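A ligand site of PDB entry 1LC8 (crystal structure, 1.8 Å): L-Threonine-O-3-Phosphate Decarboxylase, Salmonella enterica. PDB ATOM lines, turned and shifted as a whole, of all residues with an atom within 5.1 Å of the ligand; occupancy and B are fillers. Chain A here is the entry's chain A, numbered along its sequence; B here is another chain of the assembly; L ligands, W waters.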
ATOM      1  N   HIS A   8     -16.850  -0.766  18.779  1.00  0.00           N
ATOM      2  CA  HIS A   8     -16.141  -1.263  17.600  1.00  0.00           C
ATOM      3  C   HIS A   8     -16.262  -0.305  16.429  1.00  0.00           C
ATOM      4  O   HIS A   8     -17.064   0.638  16.472  1.00  0.00           O
ATOM      5  CB  HIS A   8     -16.724  -2.619  17.142  1.00  0.00           C
ATOM      6  CG  HIS A   8     -16.471  -3.722  18.110  1.00  0.00           C
ATOM      7  ND1 HIS A   8     -15.206  -4.254  18.292  1.00  0.00           N
ATOM      8  CD2 HIS A   8     -17.284  -4.409  18.936  1.00  0.00           C
ATOM      9  CE1 HIS A   8     -15.266  -5.219  19.193  1.00  0.00           C
ATOM     10  NE2 HIS A   8     -16.525  -5.341  19.595  1.00  0.00           N
ATOM     11  N   GLY A   9     -15.464  -0.565  15.402  1.00  0.00           N
ATOM     12  CA  GLY A   9     -15.502   0.250  14.203  1.00  0.00           C
ATOM     13  C   GLY A   9     -16.743  -0.089  13.399  1.00  0.00           C
ATOM     14  O   GLY A   9     -17.559  -0.926  13.770  1.00  0.00           O
ATOM     15  N   GLY A  10     -16.865   0.586  12.253  1.00  0.00           N
ATOM     16  CA  GLY A  10     -17.978   0.382  11.359  1.00  0.00           C
ATOM     17  C   GLY A  10     -19.274   1.018  11.823  1.00  0.00           C
ATOM     18  O   GLY A  10     -20.303   0.843  11.148  1.00  0.00           O
ATOM     19  N   SER A  30     -13.235   2.744   9.149  1.00  0.00           N
ATOM     20  CA  SER A  30     -13.115   2.183  10.516  1.00  0.00           C
ATOM     21  C   SER A  30     -13.448   0.686  10.635  1.00  0.00           C
ATOM     22  O   SER A  30     -13.274   0.112  11.715  1.00  0.00           O
ATOM     23  CB  SER A  30     -14.001   2.948  11.503  1.00  0.00           C
ATOM     24  OG  SER A  30     -15.356   2.667  11.208  1.00  0.00           O
ATOM     25  N   ALA A  31     -13.901   0.087   9.535  1.00  0.00           N
ATOM     26  CA  ALA A  31     -14.213  -1.343   9.461  1.00  0.00           C
ATOM     27  C   ALA A  31     -13.385  -1.762   8.256  1.00  0.00           C
ATOM     28  O   ALA A  31     -13.092  -0.927   7.404  1.00  0.00           O
ATOM     29  CB  ALA A  31     -15.719  -1.580   9.221  1.00  0.00           C
ATOM     30  N   ASN A  83     -23.109 -17.273  13.720  1.00  0.00           N
ATOM     31  CA  ASN A  83     -23.745 -15.997  13.293  1.00  0.00           C
ATOM     32  C   ASN A  83     -22.620 -14.960  13.406  1.00  0.00           C
ATOM     33  O   ASN A  83     -22.634 -14.108  14.299  1.00  0.00           O
ATOM     34  CB  ASN A  83     -24.878 -15.722  14.305  1.00  0.00           C
ATOM     35  CG  ASN A  83     -25.679 -14.482  13.993  1.00  0.00           C
ATOM     36  OD1 ASN A  83     -26.103 -13.746  14.902  1.00  0.00           O
ATOM     37  ND2 ASN A  83     -25.941 -14.266  12.720  1.00  0.00           N
ATOM     38  N   GLY A  84     -21.682 -15.027  12.450  1.00  0.00           N
ATOM     39  CA  GLY A  84     -20.505 -14.203  12.430  1.00  0.00           C
ATOM     40  C   GLY A  84     -19.449 -14.971  13.236  1.00  0.00           C
ATOM     41  O   GLY A  84     -19.822 -15.798  14.070  1.00  0.00           O
ATOM     42  N   GLU A  85     -18.168 -14.724  12.976  1.00  0.00           N
ATOM     43  CA  GLU A  85     -17.103 -15.352  13.793  1.00  0.00           C
ATOM     44  C   GLU A  85     -17.273 -14.843  15.246  1.00  0.00           C
ATOM     45  O   GLU A  85     -16.818 -15.464  16.222  1.00  0.00           O
ATOM     46  CB  GLU A  85     -15.708 -14.976  13.254  1.00  0.00           C
ATOM     47  CG  GLU A  85     -14.629 -15.745  13.999  1.00  0.00           C
ATOM     48  CD  GLU A  85     -13.225 -15.313  13.675  1.00  0.00           C
ATOM     49  OE1 GLU A  85     -12.806 -15.445  12.480  1.00  0.00           O
ATOM     50  OE2 GLU A  85     -12.526 -14.830  14.610  1.00  0.00           O
ATOM     51  N   THR A  86     -17.912 -13.676  15.393  1.00  0.00           N
ATOM     52  CA  THR A  86     -18.195 -13.170  16.750  1.00  0.00           C
ATOM     53  C   THR A  86     -18.921 -14.309  17.534  1.00  0.00           C
ATOM     54  O   THR A  86     -18.575 -14.604  18.688  1.00  0.00           O
ATOM     55  CB  THR A  86     -19.098 -11.920  16.706  1.00  0.00           C
ATOM     56  OG1 THR A  86     -18.391 -10.847  16.061  1.00  0.00           O
ATOM     57  CG2 THR A  86     -19.528 -11.495  18.117  1.00  0.00           C
ATOM     58  N   GLU A  87     -19.924 -14.946  16.928  1.00  0.00           N
ATOM     59  CA  GLU A  87     -20.586 -16.007  17.682  1.00  0.00           C
ATOM     60  C   GLU A  87     -19.639 -17.164  17.961  1.00  0.00           C
ATOM     61  O   GLU A  87     -19.663 -17.735  19.057  1.00  0.00           O
ATOM     62  CB  GLU A  87     -21.865 -16.520  16.995  1.00  0.00           C
ATOM     63  CG  GLU A  87     -22.561 -17.597  17.840  1.00  0.00           C
ATOM     64  CD  GLU A  87     -23.888 -18.092  17.247  1.00  0.00           C
ATOM     65  OE1 GLU A  87     -23.907 -18.480  16.073  1.00  0.00           O
ATOM     66  OE2 GLU A  87     -24.918 -18.120  17.949  1.00  0.00           O
ATOM     67  N   ILE A  89     -16.595 -17.063  18.638  1.00  0.00           N
ATOM     68  CA  ILE A  89     -15.716 -16.693  19.792  1.00  0.00           C
ATOM     69  C   ILE A  89     -16.487 -16.965  21.075  1.00  0.00           C
ATOM     70  O   ILE A  89     -15.940 -17.516  22.031  1.00  0.00           O
ATOM     71  CB  ILE A  89     -15.317 -15.183  19.711  1.00  0.00           C
ATOM     72  CG1 ILE A  89     -14.250 -15.005  18.618  1.00  0.00           C
ATOM     73  CG2 ILE A  89     -14.785 -14.665  21.100  1.00  0.00           C
ATOM     74  CD1 ILE A  89     -14.124 -13.565  18.106  1.00  0.00           C
ATOM     75  N   PHE A 108      -8.563  -7.910  19.739  1.00  0.00           N
ATOM     76  CA  PHE A 108      -9.999  -7.745  19.504  1.00  0.00           C
ATOM     77  C   PHE A 108     -10.702  -7.848  20.852  1.00  0.00           C
ATOM     78  O   PHE A 108     -10.439  -8.777  21.614  1.00  0.00           O
ATOM     79  CB  PHE A 108     -10.485  -8.854  18.554  1.00  0.00           C
ATOM     80  CG  PHE A 108     -11.929  -8.725  18.162  1.00  0.00           C
ATOM     81  CD1 PHE A 108     -12.439  -7.514  17.736  1.00  0.00           C
ATOM     82  CD2 PHE A 108     -12.760  -9.865  18.163  1.00  0.00           C
ATOM     83  CE1 PHE A 108     -13.769  -7.402  17.307  1.00  0.00           C
ATOM     84  CE2 PHE A 108     -14.106  -9.754  17.727  1.00  0.00           C
ATOM     85  CZ  PHE A 108     -14.595  -8.534  17.308  1.00  0.00           C
ATOM     86  N   TYR A 111     -12.802 -11.337  22.757  1.00  0.00           N
ATOM     87  CA  TYR A 111     -12.282 -12.520  23.498  1.00  0.00           C
ATOM     88  C   TYR A 111     -12.506 -12.257  25.001  1.00  0.00           C
ATOM     89  O   TYR A 111     -13.045 -13.096  25.720  1.00  0.00           O
ATOM     90  CB  TYR A 111     -10.764 -12.712  23.305  1.00  0.00           C
ATOM     91  CG  TYR A 111     -10.248 -12.584  21.879  1.00  0.00           C
ATOM     92  CD1 TYR A 111      -9.046 -11.926  21.628  1.00  0.00           C
ATOM     93  CD2 TYR A 111     -10.960 -13.111  20.787  1.00  0.00           C
ATOM     94  CE1 TYR A 111      -8.561 -11.758  20.328  1.00  0.00           C
ATOM     95  CE2 TYR A 111     -10.486 -12.946  19.468  1.00  0.00           C
ATOM     96  CZ  TYR A 111      -9.299 -12.280  19.255  1.00  0.00           C
ATOM     97  OH  TYR A 111      -8.877 -12.091  17.958  1.00  0.00           O
ATOM     98  N   CYS A 153      -4.341 -13.876  17.865  1.00  0.00           N
ATOM     99  CA  CYS A 153      -5.034 -13.384  16.680  1.00  0.00           C
ATOM    100  C   CYS A 153      -3.951 -13.315  15.587  1.00  0.00           C
ATOM    101  O   CYS A 153      -2.948 -12.634  15.764  1.00  0.00           O
ATOM    102  CB  CYS A 153      -5.604 -12.003  16.968  1.00  0.00           C
ATOM    103  SG  CYS A 153      -6.812 -11.499  15.690  1.00  0.00           S
ATOM    104  N   ASN A 157      -5.493  -7.874  15.398  1.00  0.00           N
ATOM    105  CA  ASN A 157      -6.373  -6.686  15.300  1.00  0.00           C
ATOM    106  C   ASN A 157      -5.878  -5.953  16.571  1.00  0.00           C
ATOM    107  O   ASN A 157      -6.027  -6.484  17.650  1.00  0.00           O
ATOM    108  CB  ASN A 157      -7.842  -7.129  15.501  1.00  0.00           C
ATOM    109  CG  ASN A 157      -8.800  -5.949  15.724  1.00  0.00           C
ATOM    110  OD1 ASN A 157      -8.361  -4.852  16.031  1.00  0.00           O
ATOM    111  ND2 ASN A 157     -10.121  -6.199  15.566  1.00  0.00           N
ATOM    112  N   ASP A 185      -7.313 -16.882  16.117  1.00  0.00           N
ATOM    113  CA  ASP A 185      -8.327 -16.124  15.414  1.00  0.00           C
ATOM    114  C   ASP A 185      -7.754 -15.757  14.041  1.00  0.00           C
ATOM    115  O   ASP A 185      -6.933 -14.849  13.911  1.00  0.00           O
ATOM    116  CB  ASP A 185      -8.663 -14.844  16.187  1.00  0.00           C
ATOM    117  CG  ASP A 185      -9.784 -14.049  15.535  1.00  0.00           C
ATOM    118  OD1 ASP A 185     -10.136 -14.362  14.371  1.00  0.00           O
ATOM    119  OD2 ASP A 185     -10.284 -13.114  16.184  1.00  0.00           O
ATOM    120  N   ALA A 187      -9.449 -14.560  11.505  1.00  0.00           N
ATOM    121  CA  ALA A 187     -10.432 -13.715  10.825  1.00  0.00           C
ATOM    122  C   ALA A 187      -9.917 -13.006   9.577  1.00  0.00           C
ATOM    123  O   ALA A 187     -10.664 -12.768   8.623  1.00  0.00           O
ATOM    124  CB  ALA A 187     -10.969 -12.645  11.808  1.00  0.00           C
ATOM    125  N   PHE A 188      -8.665 -12.592   9.593  1.00  0.00           N
ATOM    126  CA  PHE A 188      -8.139 -11.859   8.444  1.00  0.00           C
ATOM    127  C   PHE A 188      -7.080 -12.619   7.654  1.00  0.00           C
ATOM    128  O   PHE A 188      -6.414 -12.035   6.802  1.00  0.00           O
ATOM    129  CB  PHE A 188      -7.502 -10.554   8.927  1.00  0.00           C
ATOM    130  CG  PHE A 188      -8.493  -9.506   9.330  1.00  0.00           C
ATOM    131  CD1 PHE A 188      -8.793  -9.293  10.661  1.00  0.00           C
ATOM    132  CD2 PHE A 188      -9.103  -8.714   8.357  1.00  0.00           C
ATOM    133  CE1 PHE A 188      -9.688  -8.311  11.030  1.00  0.00           C
ATOM    134  CE2 PHE A 188     -10.006  -7.714   8.711  1.00  0.00           C
ATOM    135  CZ  PHE A 188     -10.306  -7.513  10.060  1.00  0.00           C
ATOM    136  N   SER A 213     -13.695 -16.217   9.524  1.00  0.00           N
ATOM    137  CA  SER A 213     -14.805 -15.337   9.245  1.00  0.00           C
ATOM    138  C   SER A 213     -14.931 -15.169   7.748  1.00  0.00           C
ATOM    139  O   SER A 213     -13.924 -15.162   7.027  1.00  0.00           O
ATOM    140  CB  SER A 213     -14.582 -13.968   9.887  1.00  0.00           C
ATOM    141  OG  SER A 213     -15.583 -13.071   9.430  1.00  0.00           O
ATOM    142  N   LEU A 214     -16.145 -15.076   7.259  1.00  0.00           N
ATOM    143  CA  LEU A 214     -16.319 -14.816   5.832  1.00  0.00           C
ATOM    144  C   LEU A 214     -16.733 -13.340   5.616  1.00  0.00           C
ATOM    145  O   LEU A 214     -16.803 -12.872   4.467  1.00  0.00           O
ATOM    146  CB  LEU A 214     -17.427 -15.686   5.231  1.00  0.00           C
ATOM    147  CG  LEU A 214     -16.956 -17.023   4.694  1.00  0.00           C
ATOM    148  CD1 LEU A 214     -17.028 -18.038   5.811  1.00  0.00           C
ATOM    149  CD2 LEU A 214     -17.904 -17.455   3.566  1.00  0.00           C
ATOM    150  N   THR A 215     -16.958 -12.592   6.684  1.00  0.00           N
ATOM    151  CA  THR A 215     -17.491 -11.252   6.468  1.00  0.00           C
ATOM    152  C   THR A 215     -16.570 -10.197   5.863  1.00  0.00           C
ATOM    153  O   THR A 215     -17.028  -9.362   5.070  1.00  0.00           O
ATOM    154  CB  THR A 215     -18.152 -10.695   7.744  1.00  0.00           C
ATOM    155  OG1 THR A 215     -17.170 -10.576   8.762  1.00  0.00           O
ATOM    156  CG2 THR A 215     -19.317 -11.645   8.201  1.00  0.00           C
ATOM    157  N   LYS A 216     -15.291 -10.219   6.190  1.00  0.00           N
ATOM    158  CA  LYS A 216     -14.396  -9.220   5.611  1.00  0.00           C
ATOM    159  C   LYS A 216     -13.958  -9.588   4.190  1.00  0.00           C
ATOM    160  O   LYS A 216     -14.043  -8.778   3.260  1.00  0.00           O
ATOM    161  CB  LYS A 216     -13.169  -9.011   6.493  1.00  0.00           C
ATOM    162  CG  LYS A 216     -13.523  -8.629   7.936  1.00  0.00           C
ATOM    163  CD  LYS A 216     -13.303  -9.841   8.854  1.00  0.00           C
ATOM    164  CE  LYS A 216     -13.924  -9.649  10.252  1.00  0.00           C
ATOM    165  NZ  LYS A 216     -13.780  -8.254  10.742  1.00  0.00           N
ATOM    166  N   PRO A 221     -20.460  -8.573   5.962  1.00  0.00           N
ATOM    167  CA  PRO A 221     -20.528  -8.370   7.415  1.00  0.00           C
ATOM    168  C   PRO A 221     -21.958  -8.119   7.907  1.00  0.00           C
ATOM    169  O   PRO A 221     -22.275  -8.362   9.065  1.00  0.00           O
ATOM    170  CB  PRO A 221     -19.622  -7.157   7.636  1.00  0.00           C
ATOM    171  CG  PRO A 221     -19.825  -6.359   6.385  1.00  0.00           C
ATOM    172  CD  PRO A 221     -19.704  -7.475   5.330  1.00  0.00           C
ATOM    173  N   ARG A 224     -23.633 -11.738   8.487  1.00  0.00           N
ATOM    174  CA  ARG A 224     -23.068 -12.445   9.656  1.00  0.00           C
ATOM    175  C   ARG A 224     -22.722 -13.926   9.398  1.00  0.00           C
ATOM    176  O   ARG A 224     -23.606 -14.773   9.412  1.00  0.00           O
ATOM    177  CB  ARG A 224     -24.043 -12.361  10.841  1.00  0.00           C
ATOM    178  CG  ARG A 224     -24.778 -10.997  11.077  1.00  0.00           C
ATOM    179  CD  ARG A 224     -23.793  -9.857  11.406  1.00  0.00           C
ATOM    180  NE  ARG A 224     -22.922 -10.191  12.546  1.00  0.00           N
ATOM    181  CZ  ARG A 224     -21.589 -10.269  12.458  1.00  0.00           C
ATOM    182  NH1 ARG A 224     -20.994 -10.038  11.302  1.00  0.00           N
ATOM    183  NH2 ARG A 224     -20.854 -10.615  13.517  1.00  0.00           N
ATOM    184  N   LEU A 225     -21.454 -14.235   9.174  1.00  0.00           N
ATOM    185  CA  LEU A 225     -21.108 -15.633   8.990  1.00  0.00           C
ATOM    186  C   LEU A 225     -19.652 -15.865   9.310  1.00  0.00           C
ATOM    187  O   LEU A 225     -18.754 -15.202   8.784  1.00  0.00           O
ATOM    188  CB  LEU A 225     -21.406 -16.107   7.565  1.00  0.00           C
ATOM    189  CG  LEU A 225     -21.108 -17.604   7.339  1.00  0.00           C
ATOM    190  CD1 LEU A 225     -22.127 -18.441   8.167  1.00  0.00           C
ATOM    191  CD2 LEU A 225     -21.276 -17.957   5.820  1.00  0.00           C
ATOM    192  N   GLY A 226     -19.439 -16.815  10.220  1.00  0.00           N
ATOM    193  CA  GLY A 226     -18.079 -17.226  10.566  1.00  0.00           C
ATOM    194  C   GLY A 226     -18.172 -18.707  10.929  1.00  0.00           C
ATOM    195  O   GLY A 226     -19.253 -19.324  10.823  1.00  0.00           O
ATOM    196  N   ARG A 323     -10.902   4.392  12.780  1.00  0.00           N
ATOM    197  CA  ARG A 323     -10.981   3.729  14.062  1.00  0.00           C
ATOM    198  C   ARG A 323      -9.978   4.338  15.046  1.00  0.00           C
ATOM    199  O   ARG A 323      -8.785   4.490  14.735  1.00  0.00           O
ATOM    200  CB  ARG A 323     -10.688   2.233  13.880  1.00  0.00           C
ATOM    201  CG  ARG A 323     -10.645   1.422  15.196  1.00  0.00           C
ATOM    202  CD  ARG A 323     -12.070   1.144  15.694  1.00  0.00           C
ATOM    203  NE  ARG A 323     -12.215  -0.088  16.499  1.00  0.00           N
ATOM    204  CZ  ARG A 323     -12.056  -0.185  17.822  1.00  0.00           C
ATOM    205  NH1 ARG A 323     -11.718   0.879  18.547  1.00  0.00           N
ATOM    206  NH2 ARG A 323     -12.294  -1.342  18.427  1.00  0.00           N
ATOM    207  N   TYR A 328      -8.401   0.125  23.142  1.00  0.00           N
ATOM    208  CA  TYR A 328      -7.741  -1.163  23.193  1.00  0.00           C
ATOM    209  C   TYR A 328      -6.764  -1.109  24.379  1.00  0.00           C
ATOM    210  O   TYR A 328      -5.985  -0.169  24.504  1.00  0.00           O
ATOM    211  CB  TYR A 328      -6.844  -1.411  21.969  1.00  0.00           C
ATOM    212  CG  TYR A 328      -7.591  -1.796  20.730  1.00  0.00           C
ATOM    213  CD1 TYR A 328      -7.695  -3.125  20.341  1.00  0.00           C
ATOM    214  CD2 TYR A 328      -8.169  -0.814  19.912  1.00  0.00           C
ATOM    215  CE1 TYR A 328      -8.356  -3.488  19.147  1.00  0.00           C
ATOM    216  CE2 TYR A 328      -8.836  -1.161  18.735  1.00  0.00           C
ATOM    217  CZ  TYR A 328      -8.919  -2.506  18.358  1.00  0.00           C
ATOM    218  OH  TYR A 328      -9.528  -2.868  17.159  1.00  0.00           O
ATOM    219  N   ARG A 337      -6.711   3.220  13.445  1.00  0.00           N
ATOM    220  CA  ARG A 337      -6.558   2.178  12.432  1.00  0.00           C
ATOM    221  C   ARG A 337      -7.379   2.589  11.232  1.00  0.00           C
ATOM    222  O   ARG A 337      -8.490   3.121  11.380  1.00  0.00           O
ATOM    223  CB  ARG A 337      -7.064   0.822  12.948  1.00  0.00           C
ATOM    224  CG  ARG A 337      -6.826  -0.356  11.983  1.00  0.00           C
ATOM    225  CD  ARG A 337      -7.639  -1.603  12.433  1.00  0.00           C
ATOM    226  NE  ARG A 337      -9.072  -1.323  12.344  1.00  0.00           N
ATOM    227  CZ  ARG A 337      -9.995  -1.881  13.107  1.00  0.00           C
ATOM    228  NH1 ARG A 337      -9.661  -2.783  14.037  1.00  0.00           N
ATOM    229  NH2 ARG A 337     -11.264  -1.472  13.013  1.00  0.00           N
ATOM    230  N   TYR B  56     -21.412  -3.662   8.329  1.00  0.00           N
ATOM    231  CA  TYR B  56     -21.924  -4.261   9.561  1.00  0.00           C
ATOM    232  C   TYR B  56     -23.308  -3.680   9.887  1.00  0.00           C
ATOM    233  O   TYR B  56     -23.639  -2.558   9.451  1.00  0.00           O
ATOM    234  CB  TYR B  56     -20.993  -3.929  10.743  1.00  0.00           C
ATOM    235  CG  TYR B  56     -19.886  -4.901  10.926  1.00  0.00           C
ATOM    236  CD1 TYR B  56     -18.654  -4.703  10.326  1.00  0.00           C
ATOM    237  CD2 TYR B  56     -20.093  -6.073  11.647  1.00  0.00           C
ATOM    238  CE1 TYR B  56     -17.644  -5.663  10.422  1.00  0.00           C
ATOM    239  CE2 TYR B  56     -19.116  -7.036  11.762  1.00  0.00           C
ATOM    240  CZ  TYR B  56     -17.894  -6.830  11.156  1.00  0.00           C
ATOM    241  OH  TYR B  56     -16.958  -7.826  11.286  1.00  0.00           O
ATOM    242  N   TRP B 246     -23.742  -7.196  17.127  1.00  0.00           N
ATOM    243  CA  TRP B 246     -24.225  -7.432  15.763  1.00  0.00           C
ATOM    244  C   TRP B 246     -24.981  -8.715  15.577  1.00  0.00           C
ATOM    245  O   TRP B 246     -24.937  -9.323  14.501  1.00  0.00           O
ATOM    246  CB  TRP B 246     -23.053  -7.455  14.771  1.00  0.00           C
ATOM    247  CG  TRP B 246     -22.030  -6.320  14.884  1.00  0.00           C
ATOM    248  CD1 TRP B 246     -22.202  -4.974  14.597  1.00  0.00           C
ATOM    249  CD2 TRP B 246     -20.648  -6.489  15.231  1.00  0.00           C
ATOM    250  NE1 TRP B 246     -20.985  -4.321  14.748  1.00  0.00           N
ATOM    251  CE2 TRP B 246     -20.024  -5.223  15.129  1.00  0.00           C
ATOM    252  CE3 TRP B 246     -19.882  -7.610  15.626  1.00  0.00           C
ATOM    253  CZ2 TRP B 246     -18.655  -5.036  15.397  1.00  0.00           C
ATOM    254  CZ3 TRP B 246     -18.508  -7.415  15.894  1.00  0.00           C
ATOM    255  CH2 TRP B 246     -17.926  -6.142  15.775  1.00  0.00           C
HETATM  256  N1  LIG L   1     -12.068 -11.393  14.834  1.00  0.00           N
HETATM  257  C1  LIG L   1     -11.408 -10.231  14.599  1.00  0.00           C
HETATM  258  C2  LIG L   1      -9.964 -10.155  14.774  1.00  0.00           C
HETATM  259  C3  LIG L   1     -12.220  -9.115  14.195  1.00  0.00           C
HETATM  260  O1  LIG L   1     -11.652  -7.974  13.961  1.00  0.00           O
HETATM  261  C4  LIG L   1     -13.665  -9.327  14.051  1.00  0.00           C
HETATM  262  C5  LIG L   1     -14.445  -8.159  13.639  1.00  0.00           C
HETATM  263  C6  LIG L   1     -14.253 -10.552  14.312  1.00  0.00           C
HETATM  264  C7  LIG L   1     -13.420 -11.634  14.708  1.00  0.00           C
HETATM  265  C8  LIG L   1     -15.689 -10.894  14.208  1.00  0.00           C
HETATM  266  O2  LIG L   1     -16.053 -10.919  12.818  1.00  0.00           O
HETATM  267  P1  LIG L   1     -17.497 -11.333  12.248  1.00  0.00           P
HETATM  268  O3  LIG L   1     -17.295 -12.651  11.440  1.00  0.00           O
HETATM  269  O4  LIG L   1     -18.091 -10.224  11.317  1.00  0.00           O
HETATM  270  O5  LIG L   1     -18.404 -11.629  13.468  1.00  0.00           O
HETATM  271  P2  LIG L   1     -13.083  -3.658  15.558  1.00  0.00           P
HETATM  272  O6  LIG L   1     -13.030  -3.800  17.083  1.00  0.00           O
HETATM  273  O7  LIG L   1     -13.189  -2.169  15.148  1.00  0.00           O
HETATM  274  O8  LIG L   1     -11.815  -4.267  14.938  1.00  0.00           O
HETATM  275  N2  LIG L   1     -14.332  -6.895  13.698  1.00  0.00           N
HETATM  276  C9  LIG L   1     -15.159  -5.801  13.239  1.00  0.00           C
HETATM  277  C10 LIG L   1     -14.549  -4.460  13.611  1.00  0.00           C
HETATM  278  O9  LIG L   1     -14.349  -4.457  15.043  1.00  0.00           O
HETATM  279  C11 LIG L   1     -15.530  -3.396  13.200  1.00  0.00           C
HETATM  280  O   HOH W   1     -11.083  -5.327  12.572  1.00  0.00           O
HETATM  281  O   HOH W   2     -13.518  -5.330  10.208  1.00  0.00           O
HETATM  282  O   HOH W   3     -11.827  -4.606  19.465  1.00  0.00           O
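ND1 of His 8 lies within hydrogen-bond range of O6 of the ligand (2.5 Å).
The side-chain amide nitrogen of Asn 157 sits at hydrogen-bond distance from an oxygen (O8) of the ligand (2.6 Å).
An oxygen (O5) of the ligand is in salt-bridge range of the guanidinium group (NH2) of Arg 224, at 2.7 Å.
The side-chain hydroxyl (OH) of Tyr 56 of chain B sits at hydrogen-bond distance from an oxygen (O4) of the ligand (2.7 Å).
An oxygen (O7) of the ligand is in salt-bridge range of the guanidinium group (NE) of Arg 323, at 2.7 Å.
An oxygen (O3) of the ligand sits at hydrogen-bond distance from the side-chain hydroxyl of Ser 213.
N of Thr 86 lies within hydrogen-bond range of O5 of the ligand.
An oxygen (O5) of the ligand lies within hydrogen-bond range of the side-chain hydroxyl (OG1) of Thr 86 (2.7 Å).
The backbone NH (N) of Glu 85 is in hydrogen-bond range of an oxygen (O3) of the ligand, at 2.7 Å.
The side-chain hydroxyl (OG1) of Thr 215 sits at hydrogen-bond distance from an oxygen (O4) of the ligand (2.7 Å).
The guanidinium group of Arg 337 is in salt-bridge range of an oxygen (O8) of the ligand (2.8 Å).
The backbone NH (N) of Gly 9 lies within hydrogen-bond range of an oxygen (O7) of the ligand.
The side-chain carboxylate of Asp 185 lies within hydrogen-bond range of a nitrogen (N1) of the ligand (2.8 Å).
The side-chain amino group (NZ) of Lys 216 lies close to a nitrogen (N2) of the ligand (3.3 Å).
OH of Tyr 328 lies within hydrogen-bond range of O8 of the ligand, at 3.5 Å.
OH of Tyr 328 is in hydrogen-bond range of OD1 of Asn 157 (2.6 Å).
O of Trp 246 of chain B sits at hydrogen-bond distance from NE of Arg 224.
The guanidinium group of Arg 323 lies within hydrogen-bond range of the side-chain hydroxyl of Tyr 328 (3.4 Å).
The backbone NH of Ser 213 sits at hydrogen-bond distance from the side-chain carboxylate of Glu 85, 3.2 Å away.
The side-chain hydroxyl (OG) of Ser 213 is in hydrogen-bond range of the side-chain hydroxyl (OG1) of Thr 215.
The side-chain sulfur (SG) of Cys 153 sits close to the backbone carbonyl oxygen (O) of Asp 185 (3.8 Å).
The side-chain carboxylate (OD2) of Asp 185 lies within hydrogen-bond range of the side-chain hydroxyl (OH) of Tyr 111 (2.5 Å).
OH of Tyr 111 is in hydrogen-bond range of SG of Cys 153 (3.1 Å).
Gly 84 touches the ligand.
CD1 of Ile 89 touches C7 of the ligand, at 3.97 Å.
Phe 108 touches the ligand.
OH of Tyr 111 touches C2 of the ligand, 3.9 Å away.
Cys 153 touches the ligand.
Ala 187 touches the ligand (CB to N1, 3.5 Å).
Phe 188 touches the ligand.
O of Leu 225 touches O3 of the ligand, at 3.96 Å.
Trp 246 of chain B touches the ligand.
23 residues have an atom within 4 Å of the ligand: His 8, Gly 9, Gly 84, Glu 85, Thr 86, Ile 89, Phe 108, Tyr 111, Cys 153, Asn 157, Asp 185, Ala 187, Phe 188, Ser 213, Thr 215, Lys 216, Arg 224, Leu 225, Arg 323, Tyr 328, Arg 337, Tyr 56 of chain B and Trp 246 of chain B.
The nearest printed residue that does not touch the ligand is Ser 30 (4.1 Å).
Water W1 lies within hydrogen-bond range of O8 of the ligand (2.7 Å), NH1 of Arg 337 (3.3 Å) and ND2 of Asn 157 (3.3 Å).
Water W3 lies within hydrogen-bond range of an oxygen (O6) of the ligand (2.8 Å) and the guanidinium group of Arg 323 (3.5 Å).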
